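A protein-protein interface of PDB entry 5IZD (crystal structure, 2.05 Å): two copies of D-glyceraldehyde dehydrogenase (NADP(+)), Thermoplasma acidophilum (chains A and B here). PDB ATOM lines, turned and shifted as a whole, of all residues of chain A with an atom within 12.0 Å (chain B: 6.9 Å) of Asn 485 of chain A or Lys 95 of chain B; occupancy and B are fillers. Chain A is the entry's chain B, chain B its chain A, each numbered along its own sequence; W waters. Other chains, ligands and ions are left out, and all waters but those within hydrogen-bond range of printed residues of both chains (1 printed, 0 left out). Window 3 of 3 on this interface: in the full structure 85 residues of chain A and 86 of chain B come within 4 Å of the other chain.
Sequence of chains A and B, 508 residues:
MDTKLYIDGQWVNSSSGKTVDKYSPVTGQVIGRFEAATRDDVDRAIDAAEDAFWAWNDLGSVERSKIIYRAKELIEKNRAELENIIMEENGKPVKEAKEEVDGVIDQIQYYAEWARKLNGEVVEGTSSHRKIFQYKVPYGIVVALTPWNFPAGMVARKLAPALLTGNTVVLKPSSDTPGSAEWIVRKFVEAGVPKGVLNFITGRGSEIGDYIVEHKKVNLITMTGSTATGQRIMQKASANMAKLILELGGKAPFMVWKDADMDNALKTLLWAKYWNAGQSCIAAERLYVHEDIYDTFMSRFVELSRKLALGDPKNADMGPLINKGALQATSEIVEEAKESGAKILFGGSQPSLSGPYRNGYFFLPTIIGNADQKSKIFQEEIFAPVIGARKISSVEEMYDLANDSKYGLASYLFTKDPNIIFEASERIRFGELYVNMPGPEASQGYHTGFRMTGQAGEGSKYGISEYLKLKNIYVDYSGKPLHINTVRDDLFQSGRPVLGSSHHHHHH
Lys 95 of chain B touches just these residues of chain A: Asn 485 (3.6 Å) and Thr 486 (3.9 Å). No residue of chain A comes within 4 Å of Pro 93 of chain B. No residue of chain A comes within 4 Å of Val 94 of chain B. No residue of chain A comes within 4 Å of Glu 96 of chain B. No residue of chain A comes within 4 Å of Ala 97 of chain B. Glu 99 of chain B touches just one residue of chain A: Thr 486 (3.6 Å). Of the printed residues of chain B, Thr 486 of chain A touches Lys 95 (3.9 Å), Glu 99 (3.6 Å), Trp 271 (3.8 Å) and Trp 275 (3.8 Å). Printed residues of chain B within 4 Å of Ile 484 of chain A: Trp 271 (3.7 Å). Of the printed residues of chain A, Trp 275 of chain B touches Thr 486. Of the printed residues of chain A, Trp 271 of chain B touches Ile 484 and Thr 486. Pro 481 of chain A touches none of the printed residues of chain B. Arg 488 of chain A touches none of the printed residues of chain B. The nearest residue of chain B that does not touch Asn 485 of chain A is Glu 99 of chain B (4.5 Å). The nearest printed residue of chain A that does not touch Trp 271 of chain B is Val 487 of chain A (4.03 Å).
Water W1 lies within hydrogen-bond range of OG1 of Thr 486 of chain A (2.8 Å), OE2 of Glu 99 of chain B (2.9 Å) and NE1 of Trp 271 of chain B (3.4 Å).
No position is printed for both chains.
NE1 of Trp 275 of chain B lies within hydrogen-bond range of OE2 of Glu 99 of chain B, 3.2 Å away.
Printed residues of chain A that touch a printed residue of chain B: Ile 484, Asn 485 and Thr 486. Hydrophobic or aromatic side chains of chain A within 4 Å of the printed part of chain B: Ile 484. Hydrophobic or aromatic side chains of chain B within 4 Å of the printed part of chain A: Trp 271 and Trp 275. Among the printed residues, 6 pairs touch across the chains. Among the printed residues, no Asp or Glu carboxylate lies within 4 Å of a Lys or Arg side-chain nitrogen of the other chain.
Among the printed residues, merely in contact across the chains: Thr 486 of chain A with Glu 99 of chain B (3.6 Å), Asn 485 of chain A with Lys 95 of chain B (3.6 Å), Ile 484 of chain A with Trp 271 of chain B (3.7 Å), Thr 486 of chain A with Trp 271 of chain B (3.8 Å), Thr 486 of chain A with Trp 275 of chain B (3.8 Å) and Thr 486 of chain A with Lys 95 of chain B (3.9 Å).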
ATOM      1  N   THR A 126     -17.688  22.251 -21.707  1.00  0.00           N
ATOM      2  CA  THR A 126     -18.466  21.249 -22.469  1.00  0.00           C
ATOM      3  C   THR A 126     -19.626  21.857 -23.238  1.00  0.00           C
ATOM      4  O   THR A 126     -20.456  21.145 -23.750  1.00  0.00           O
ATOM      5  CB  THR A 126     -18.978  20.150 -21.525  1.00  0.00           C
ATOM      6  OG1 THR A 126     -19.636  20.736 -20.404  1.00  0.00           O
ATOM      7  CG2 THR A 126     -17.801  19.405 -20.984  1.00  0.00           C
ATOM      8  N   ARG A 130     -20.066  27.492 -21.225  1.00  0.00           N
ATOM      9  CA  ARG A 130     -19.245  27.012 -20.123  1.00  0.00           C
ATOM     10  C   ARG A 130     -17.744  27.292 -20.374  1.00  0.00           C
ATOM     11  O   ARG A 130     -17.269  27.244 -21.480  1.00  0.00           O
ATOM     12  CB  ARG A 130     -19.458  25.513 -19.922  1.00  0.00           C
ATOM     13  CG  ARG A 130     -20.848  25.171 -19.374  1.00  0.00           C
ATOM     14  CD  ARG A 130     -21.097  23.662 -19.363  1.00  0.00           C
ATOM     15  NE  ARG A 130     -22.326  23.403 -18.619  1.00  0.00           N
ATOM     16  CZ  ARG A 130     -22.736  22.179 -18.259  1.00  0.00           C
ATOM     17  NH1 ARG A 130     -22.020  21.099 -18.587  1.00  0.00           N
ATOM     18  NH2 ARG A 130     -23.863  22.041 -17.577  1.00  0.00           N
ATOM     19  N   ASP A 476     -20.993  27.614 -15.566  1.00  0.00           N
ATOM     20  CA  ASP A 476     -22.094  27.605 -16.557  1.00  0.00           C
ATOM     21  C   ASP A 476     -22.797  28.961 -16.433  1.00  0.00           C
ATOM     22  O   ASP A 476     -23.346  29.307 -15.392  1.00  0.00           O
ATOM     23  CB  ASP A 476     -23.091  26.511 -16.268  1.00  0.00           C
ATOM     24  CG  ASP A 476     -24.172  26.331 -17.369  1.00  0.00           C
ATOM     25  OD1 ASP A 476     -24.963  27.273 -17.655  1.00  0.00           O
ATOM     26  OD2 ASP A 476     -24.282  25.202 -17.902  1.00  0.00           O
ATOM     27  N   PRO A 481     -32.346  26.465 -18.100  1.00  0.00           N
ATOM     28  CA  PRO A 481     -32.428  25.227 -17.284  1.00  0.00           C
ATOM     29  C   PRO A 481     -31.361  24.238 -17.686  1.00  0.00           C
ATOM     30  O   PRO A 481     -31.046  24.134 -18.865  1.00  0.00           O
ATOM     31  CB  PRO A 481     -33.827  24.665 -17.594  1.00  0.00           C
ATOM     32  CG  PRO A 481     -34.611  25.857 -18.091  1.00  0.00           C
ATOM     33  CD  PRO A 481     -33.621  26.807 -18.758  1.00  0.00           C
ATOM     34  N   LEU A 482     -30.796  23.541 -16.691  1.00  0.00           N
ATOM     35  CA  LEU A 482     -29.806  22.507 -16.925  1.00  0.00           C
ATOM     36  C   LEU A 482     -30.523  21.317 -17.490  1.00  0.00           C
ATOM     37  O   LEU A 482     -31.685  21.064 -17.117  1.00  0.00           O
ATOM     38  CB  LEU A 482     -29.129  22.121 -15.614  1.00  0.00           C
ATOM     39  CG  LEU A 482     -28.204  23.228 -15.076  1.00  0.00           C
ATOM     40  CD1 LEU A 482     -27.845  22.899 -13.643  1.00  0.00           C
ATOM     41  CD2 LEU A 482     -26.956  23.427 -15.927  1.00  0.00           C
ATOM     42  N   HIS A 483     -29.876  20.575 -18.375  1.00  0.00           N
ATOM     43  CA  HIS A 483     -30.345  19.228 -18.693  1.00  0.00           C
ATOM     44  C   HIS A 483     -29.200  18.311 -18.317  1.00  0.00           C
ATOM     45  O   HIS A 483     -28.059  18.511 -18.728  1.00  0.00           O
ATOM     46  CB  HIS A 483     -30.839  19.091 -20.143  1.00  0.00           C
ATOM     47  CG  HIS A 483     -31.909  20.092 -20.488  1.00  0.00           C
ATOM     48  ND1 HIS A 483     -33.243  19.921 -20.142  1.00  0.00           N
ATOM     49  CD2 HIS A 483     -31.829  21.309 -21.082  1.00  0.00           C
ATOM     50  CE1 HIS A 483     -33.939  20.976 -20.535  1.00  0.00           C
ATOM     51  NE2 HIS A 483     -33.101  21.839 -21.096  1.00  0.00           N
ATOM     52  N   ILE A 484     -29.511  17.378 -17.417  1.00  0.00           N
ATOM     53  CA  ILE A 484     -28.558  16.377 -16.939  1.00  0.00           C
ATOM     54  C   ILE A 484     -29.094  15.016 -17.387  1.00  0.00           C
ATOM     55  O   ILE A 484     -30.247  14.656 -17.124  1.00  0.00           O
ATOM     56  CB  ILE A 484     -28.384  16.429 -15.403  1.00  0.00           C
ATOM     57  CG1 ILE A 484     -27.903  17.817 -14.946  1.00  0.00           C
ATOM     58  CG2 ILE A 484     -27.421  15.324 -14.917  1.00  0.00           C
ATOM     59  CD1 ILE A 484     -27.849  18.001 -13.448  1.00  0.00           C
ATOM     60  N   ASN A 485     -28.211  14.271 -18.035  1.00  0.00           N
ATOM     61  CA  ASN A 485     -28.603  13.095 -18.818  1.00  0.00           C
ATOM     62  C   ASN A 485     -29.287  11.978 -17.991  1.00  0.00           C
ATOM     63  O   ASN A 485     -30.241  11.365 -18.453  1.00  0.00           O
ATOM     64  CB  ASN A 485     -27.385  12.588 -19.585  1.00  0.00           C
ATOM     65  CG  ASN A 485     -27.652  11.295 -20.321  1.00  0.00           C
ATOM     66  OD1 ASN A 485     -28.734  11.097 -20.934  1.00  0.00           O
ATOM     67  ND2 ASN A 485     -26.718  10.354 -20.198  1.00  0.00           N
ATOM     68  N   THR A 486     -28.782  11.746 -16.783  1.00  0.00           N
ATOM     69  CA  THR A 486     -29.305  10.759 -15.831  1.00  0.00           C
ATOM     70  C   THR A 486     -30.321  11.289 -14.780  1.00  0.00           C
ATOM     71  O   THR A 486     -30.671  10.570 -13.849  1.00  0.00           O
ATOM     72  CB  THR A 486     -28.112  10.091 -15.099  1.00  0.00           C
ATOM     73  OG1 THR A 486     -27.358  11.110 -14.410  1.00  0.00           O
ATOM     74  CG2 THR A 486     -27.192   9.394 -16.096  1.00  0.00           C
ATOM     75  N   VAL A 487     -30.780  12.534 -14.918  1.00  0.00           N
ATOM     76  CA  VAL A 487     -31.787  13.116 -14.025  1.00  0.00           C
ATOM     77  C   VAL A 487     -32.973  13.335 -14.931  1.00  0.00           C
ATOM     78  O   VAL A 487     -32.892  14.142 -15.841  1.00  0.00           O
ATOM     79  CB  VAL A 487     -31.300  14.448 -13.386  1.00  0.00           C
ATOM     80  CG1 VAL A 487     -32.375  15.074 -12.504  1.00  0.00           C
ATOM     81  CG2 VAL A 487     -30.026  14.203 -12.591  1.00  0.00           C
ATOM     82  N   ARG A 488     -34.040  12.579 -14.707  1.00  0.00           N
ATOM     83  CA  ARG A 488     -35.215  12.668 -15.532  1.00  0.00           C
ATOM     84  C   ARG A 488     -35.784  14.038 -15.419  1.00  0.00           C
ATOM     85  O   ARG A 488     -35.955  14.536 -14.346  1.00  0.00           O
ATOM     86  CB  ARG A 488     -36.259  11.635 -15.105  1.00  0.00           C
ATOM     87  CG  ARG A 488     -35.869  10.200 -15.405  1.00  0.00           C
ATOM     88  CD  ARG A 488     -36.998   9.245 -15.071  1.00  0.00           C
ATOM     89  NE  ARG A 488     -37.055   9.002 -13.656  1.00  0.00           N
ATOM     90  CZ  ARG A 488     -38.062   9.351 -12.894  1.00  0.00           C
ATOM     91  NH1 ARG A 488     -39.100   9.943 -13.423  1.00  0.00           N
ATOM     92  NH2 ARG A 488     -38.027   9.105 -11.609  1.00  0.00           N
ATOM     93  N   ASP A 489     -36.021  14.651 -16.547  1.00  0.00           N
ATOM     94  CA  ASP A 489     -36.596  15.963 -16.617  1.00  0.00           C
ATOM     95  C   ASP A 489     -38.030  15.895 -16.091  1.00  0.00           C
ATOM     96  O   ASP A 489     -38.575  16.853 -15.577  1.00  0.00           O
ATOM     97  CB  ASP A 489     -36.565  16.428 -18.058  1.00  0.00           C
ATOM     98  N   ASP A 490     -38.589  14.701 -16.160  1.00  0.00           N
ATOM     99  CA  ASP A 490     -39.948  14.412 -15.770  1.00  0.00           C
ATOM    100  C   ASP A 490     -40.177  14.773 -14.325  1.00  0.00           C
ATOM    101  O   ASP A 490     -41.290  14.795 -13.884  1.00  0.00           O
ATOM    102  N   LEU A 491     -39.116  14.997 -13.576  1.00  0.00           N
ATOM    103  CA  LEU A 491     -39.214  15.419 -12.207  1.00  0.00           C
ATOM    104  C   LEU A 491     -39.387  16.924 -12.042  1.00  0.00           C
ATOM    105  O   LEU A 491     -39.714  17.373 -10.962  1.00  0.00           O
ATOM    106  CB  LEU A 491     -37.957  15.012 -11.471  1.00  0.00           C
ATOM    107  CG  LEU A 491     -37.688  13.542 -11.418  1.00  0.00           C
ATOM    108  CD1 LEU A 491     -36.256  13.269 -11.065  1.00  0.00           C
ATOM    109  CD2 LEU A 491     -38.603  12.886 -10.423  1.00  0.00           C
ATOM    110  N   PHE A 492     -39.160  17.698 -13.096  1.00  0.00           N
ATOM    111  CA  PHE A 492     -39.224  19.139 -13.003  1.00  0.00           C
ATOM    112  C   PHE A 492     -40.081  19.712 -14.117  1.00  0.00           C
ATOM    113  O   PHE A 492     -41.084  19.140 -14.500  1.00  0.00           O
ATOM    114  CB  PHE A 492     -37.812  19.752 -13.089  1.00  0.00           C
ATOM    115  CG  PHE A 492     -36.892  19.396 -11.947  1.00  0.00           C
ATOM    116  CD1 PHE A 492     -36.080  18.303 -12.029  1.00  0.00           C
ATOM    117  CD2 PHE A 492     -36.805  20.202 -10.834  1.00  0.00           C
ATOM    118  CE1 PHE A 492     -35.237  17.981 -11.011  1.00  0.00           C
ATOM    119  CE2 PHE A 492     -35.964  19.892  -9.811  1.00  0.00           C
ATOM    120  CZ  PHE A 492     -35.177  18.773  -9.904  1.00  0.00           C
ATOM    121  N   MET B  87     -22.820  -2.907 -16.238  1.00  0.00           N
ATOM    122  CA  MET B  87     -24.129  -3.109 -15.613  1.00  0.00           C
ATOM    123  C   MET B  87     -24.112  -4.362 -14.788  1.00  0.00           C
ATOM    124  O   MET B  87     -24.650  -4.357 -13.692  1.00  0.00           O
ATOM    125  CB  MET B  87     -25.298  -3.109 -16.609  1.00  0.00           C
ATOM    126  CG  MET B  87     -25.484  -1.729 -17.285  1.00  0.00           C
ATOM    127  SD  MET B  87     -26.992  -1.761 -18.297  1.00  0.00           S
ATOM    128  CE  MET B  87     -26.355  -2.623 -19.737  1.00  0.00           C
ATOM    129  N   LYS B  92     -24.786  -0.586 -12.287  1.00  0.00           N
ATOM    130  CA  LYS B  92     -25.078   0.806 -12.704  1.00  0.00           C
ATOM    131  C   LYS B  92     -26.320   0.918 -13.581  1.00  0.00           C
ATOM    132  O   LYS B  92     -26.531   0.077 -14.481  1.00  0.00           O
ATOM    133  CB  LYS B  92     -23.942   1.413 -13.524  1.00  0.00           C
ATOM    134  CG  LYS B  92     -22.628   1.529 -12.791  1.00  0.00           C
ATOM    135  CD  LYS B  92     -21.786   2.721 -13.238  1.00  0.00           C
ATOM    136  CE  LYS B  92     -20.439   2.621 -12.552  1.00  0.00           C
ATOM    137  NZ  LYS B  92     -19.645   3.817 -12.796  1.00  0.00           N
ATOM    138  N   PRO B  93     -27.144   1.953 -13.343  1.00  0.00           N
ATOM    139  CA  PRO B  93     -28.201   2.187 -14.332  1.00  0.00           C
ATOM    140  C   PRO B  93     -27.669   2.329 -15.771  1.00  0.00           C
ATOM    141  O   PRO B  93     -26.553   2.867 -15.976  1.00  0.00           O
ATOM    142  CB  PRO B  93     -28.815   3.488 -13.847  1.00  0.00           C
ATOM    143  CG  PRO B  93     -28.672   3.426 -12.360  1.00  0.00           C
ATOM    144  CD  PRO B  93     -27.286   2.880 -12.206  1.00  0.00           C
ATOM    145  N   VAL B  94     -28.438   1.795 -16.731  1.00  0.00           N
ATOM    146  CA  VAL B  94     -28.033   1.774 -18.162  1.00  0.00           C
ATOM    147  C   VAL B  94     -27.447   3.134 -18.667  1.00  0.00           C
ATOM    148  O   VAL B  94     -26.384   3.153 -19.307  1.00  0.00           O
ATOM    149  CB  VAL B  94     -29.162   1.212 -19.098  1.00  0.00           C
ATOM    150  CG1 VAL B  94     -30.422   2.083 -19.097  1.00  0.00           C
ATOM    151  CG2 VAL B  94     -28.642   0.938 -20.520  1.00  0.00           C
ATOM    152  N   LYS B  95     -28.092   4.255 -18.342  1.00  0.00           N
ATOM    153  CA  LYS B  95     -27.574   5.552 -18.787  1.00  0.00           C
ATOM    154  C   LYS B  95     -26.201   5.869 -18.169  1.00  0.00           C
ATOM    155  O   LYS B  95     -25.363   6.518 -18.811  1.00  0.00           O
ATOM    156  CB  LYS B  95     -28.603   6.668 -18.498  1.00  0.00           C
ATOM    157  CG  LYS B  95     -29.872   6.634 -19.361  1.00  0.00           C
ATOM    158  CD  LYS B  95     -30.770   7.862 -19.172  1.00  0.00           C
ATOM    159  N   GLU B  96     -25.978   5.451 -16.917  1.00  0.00           N
ATOM    160  CA  GLU B  96     -24.658   5.566 -16.285  1.00  0.00           C
ATOM    161  C   GLU B  96     -23.613   4.679 -16.936  1.00  0.00           C
ATOM    162  O   GLU B  96     -22.449   5.075 -17.110  1.00  0.00           O
ATOM    163  CB  GLU B  96     -24.709   5.296 -14.790  1.00  0.00           C
ATOM    164  CG  GLU B  96     -25.212   6.486 -13.964  1.00  0.00           C
ATOM    165  CD  GLU B  96     -25.224   6.209 -12.447  1.00  0.00           C
ATOM    166  OE1 GLU B  96     -24.241   5.620 -11.939  1.00  0.00           O
ATOM    167  OE2 GLU B  96     -26.218   6.566 -11.748  1.00  0.00           O
ATOM    168  N   ALA B  97     -24.020   3.482 -17.311  1.00  0.00           N
ATOM    169  CA  ALA B  97     -23.118   2.558 -18.004  1.00  0.00           C
ATOM    170  C   ALA B  97     -22.763   3.138 -19.380  1.00  0.00           C
ATOM    171  O   ALA B  97     -21.595   3.158 -19.743  1.00  0.00           O
ATOM    172  CB  ALA B  97     -23.736   1.145 -18.149  1.00  0.00           C
ATOM    173  N   LYS B  98     -23.738   3.633 -20.124  1.00  0.00           N
ATOM    174  CA  LYS B  98     -23.456   4.222 -21.450  1.00  0.00           C
ATOM    175  C   LYS B  98     -22.583   5.507 -21.353  1.00  0.00           C
ATOM    176  O   LYS B  98     -21.666   5.680 -22.119  1.00  0.00           O
ATOM    177  CB  LYS B  98     -24.754   4.488 -22.220  1.00  0.00           C
ATOM    178  CG  LYS B  98     -25.452   3.208 -22.602  1.00  0.00           C
ATOM    179  CD  LYS B  98     -26.743   3.425 -23.364  1.00  0.00           C
ATOM    180  CE  LYS B  98     -27.235   2.075 -23.849  1.00  0.00           C
ATOM    181  NZ  LYS B  98     -28.464   2.251 -24.640  1.00  0.00           N
ATOM    182  N   GLU B  99     -22.869   6.345 -20.358  1.00  0.00           N
ATOM    183  CA  GLU B  99     -22.093   7.546 -20.109  1.00  0.00           C
ATOM    184  C   GLU B  99     -20.627   7.210 -19.767  1.00  0.00           C
ATOM    185  O   GLU B  99     -19.718   7.826 -20.300  1.00  0.00           O
ATOM    186  CB  GLU B  99     -22.792   8.414 -19.041  1.00  0.00           C
ATOM    187  CG  GLU B  99     -21.916   9.323 -18.255  1.00  0.00           C
ATOM    188  CD  GLU B  99     -22.714  10.252 -17.353  1.00  0.00           C
ATOM    189  OE1 GLU B  99     -22.276  11.425 -17.250  1.00  0.00           O
ATOM    190  OE2 GLU B  99     -23.710   9.812 -16.738  1.00  0.00           O
ATOM    191  N   GLU B 100     -20.400   6.186 -18.967  1.00  0.00           N
ATOM    192  CA  GLU B 100     -19.055   5.784 -18.648  1.00  0.00           C
ATOM    193  C   GLU B 100     -18.254   5.357 -19.872  1.00  0.00           C
ATOM    194  O   GLU B 100     -17.102   5.682 -20.003  1.00  0.00           O
ATOM    195  CB  GLU B 100     -19.010   4.735 -17.560  1.00  0.00           C
ATOM    196  CG  GLU B 100     -17.594   4.398 -17.184  1.00  0.00           C
ATOM    197  CD  GLU B 100     -17.446   3.656 -15.894  1.00  0.00           C
ATOM    198  OE1 GLU B 100     -18.429   3.422 -15.194  1.00  0.00           O
ATOM    199  OE2 GLU B 100     -16.331   3.303 -15.586  1.00  0.00           O
ATOM    200  N   ASP B 102     -18.924   6.314 -22.964  1.00  0.00           N
ATOM    201  CA  ASP B 102     -18.775   7.511 -23.740  1.00  0.00           C
ATOM    202  C   ASP B 102     -17.438   8.144 -23.291  1.00  0.00           C
ATOM    203  O   ASP B 102     -16.632   8.531 -24.073  1.00  0.00           O
ATOM    204  CB  ASP B 102     -19.898   8.478 -23.401  1.00  0.00           C
ATOM    205  CG  ASP B 102     -21.158   8.253 -24.210  1.00  0.00           C
ATOM    206  OD1 ASP B 102     -21.158   7.432 -25.105  1.00  0.00           O
ATOM    207  OD2 ASP B 102     -22.146   8.931 -23.965  1.00  0.00           O
ATOM    208  N   TRP B 271     -28.125  14.813  -9.073  1.00  0.00           N
ATOM    209  CA  TRP B 271     -26.948  14.262  -9.742  1.00  0.00           C
ATOM    210  C   TRP B 271     -25.773  14.028  -8.755  1.00  0.00           C
ATOM    211  O   TRP B 271     -25.273  12.887  -8.609  1.00  0.00           O
ATOM    212  CB  TRP B 271     -26.478  15.133 -10.914  1.00  0.00           C
ATOM    213  CG  TRP B 271     -25.270  14.530 -11.518  1.00  0.00           C
ATOM    214  CD1 TRP B 271     -25.232  13.554 -12.487  1.00  0.00           C
ATOM    215  CD2 TRP B 271     -23.910  14.808 -11.175  1.00  0.00           C
ATOM    216  NE1 TRP B 271     -23.937  13.200 -12.741  1.00  0.00           N
ATOM    217  CE2 TRP B 271     -23.108  13.935 -11.929  1.00  0.00           C
ATOM    218  CE3 TRP B 271     -23.291  15.673 -10.261  1.00  0.00           C
ATOM    219  CZ2 TRP B 271     -21.732  13.931 -11.825  1.00  0.00           C
ATOM    220  CZ3 TRP B 271     -21.894  15.639 -10.144  1.00  0.00           C
ATOM    221  CH2 TRP B 271     -21.151  14.786 -10.924  1.00  0.00           C
ATOM    222  N   TRP B 275     -25.858  10.015  -8.304  1.00  0.00           N
ATOM    223  CA  TRP B 275     -25.127   9.421  -9.414  1.00  0.00           C
ATOM    224  C   TRP B 275     -24.191   8.394  -8.843  1.00  0.00           C
ATOM    225  O   TRP B 275     -23.550   8.644  -7.829  1.00  0.00           O
ATOM    226  CB  TRP B 275     -24.378  10.473 -10.153  1.00  0.00           C
ATOM    227  CG  TRP B 275     -23.683  10.136 -11.444  1.00  0.00           C
ATOM    228  CD1 TRP B 275     -24.256   9.704 -12.631  1.00  0.00           C
ATOM    229  CD2 TRP B 275     -22.289  10.288 -11.715  1.00  0.00           C
ATOM    230  NE1 TRP B 275     -23.292   9.610 -13.614  1.00  0.00           N
ATOM    231  CE2 TRP B 275     -22.085   9.984 -13.085  1.00  0.00           C
ATOM    232  CE3 TRP B 275     -21.192  10.692 -10.946  1.00  0.00           C
ATOM    233  CZ2 TRP B 275     -20.833  10.066 -13.687  1.00  0.00           C
ATOM    234  CZ3 TRP B 275     -19.913  10.783 -11.569  1.00  0.00           C
ATOM    235  CH2 TRP B 275     -19.761  10.464 -12.912  1.00  0.00           C
ATOM    236  N   PRO B 313     -30.761  -2.457 -13.425  1.00  0.00           N
ATOM    237  CA  PRO B 313     -30.110  -1.404 -14.290  1.00  0.00           C
ATOM    238  C   PRO B 313     -30.898  -0.967 -15.522  1.00  0.00           C
ATOM    239  O   PRO B 313     -30.783   0.200 -15.922  1.00  0.00           O
ATOM    240  CB  PRO B 313     -28.814  -2.068 -14.730  1.00  0.00           C
ATOM    241  CG  PRO B 313     -28.468  -2.966 -13.590  1.00  0.00           C
ATOM    242  CD  PRO B 313     -29.785  -3.528 -13.078  1.00  0.00           C
ATOM    243  N   ALA B 316     -33.766   1.288 -13.202  1.00  0.00           N
ATOM    244  CA  ALA B 316     -33.577   2.015 -11.979  1.00  0.00           C
ATOM    245  C   ALA B 316     -32.972   3.342 -12.294  1.00  0.00           C
ATOM    246  O   ALA B 316     -32.244   3.472 -13.298  1.00  0.00           O
ATOM    247  CB  ALA B 316     -32.648   1.262 -11.056  1.00  0.00           C
HETATM  248  O   HOH W   1     -25.116  12.172 -15.771  1.00  0.00           O
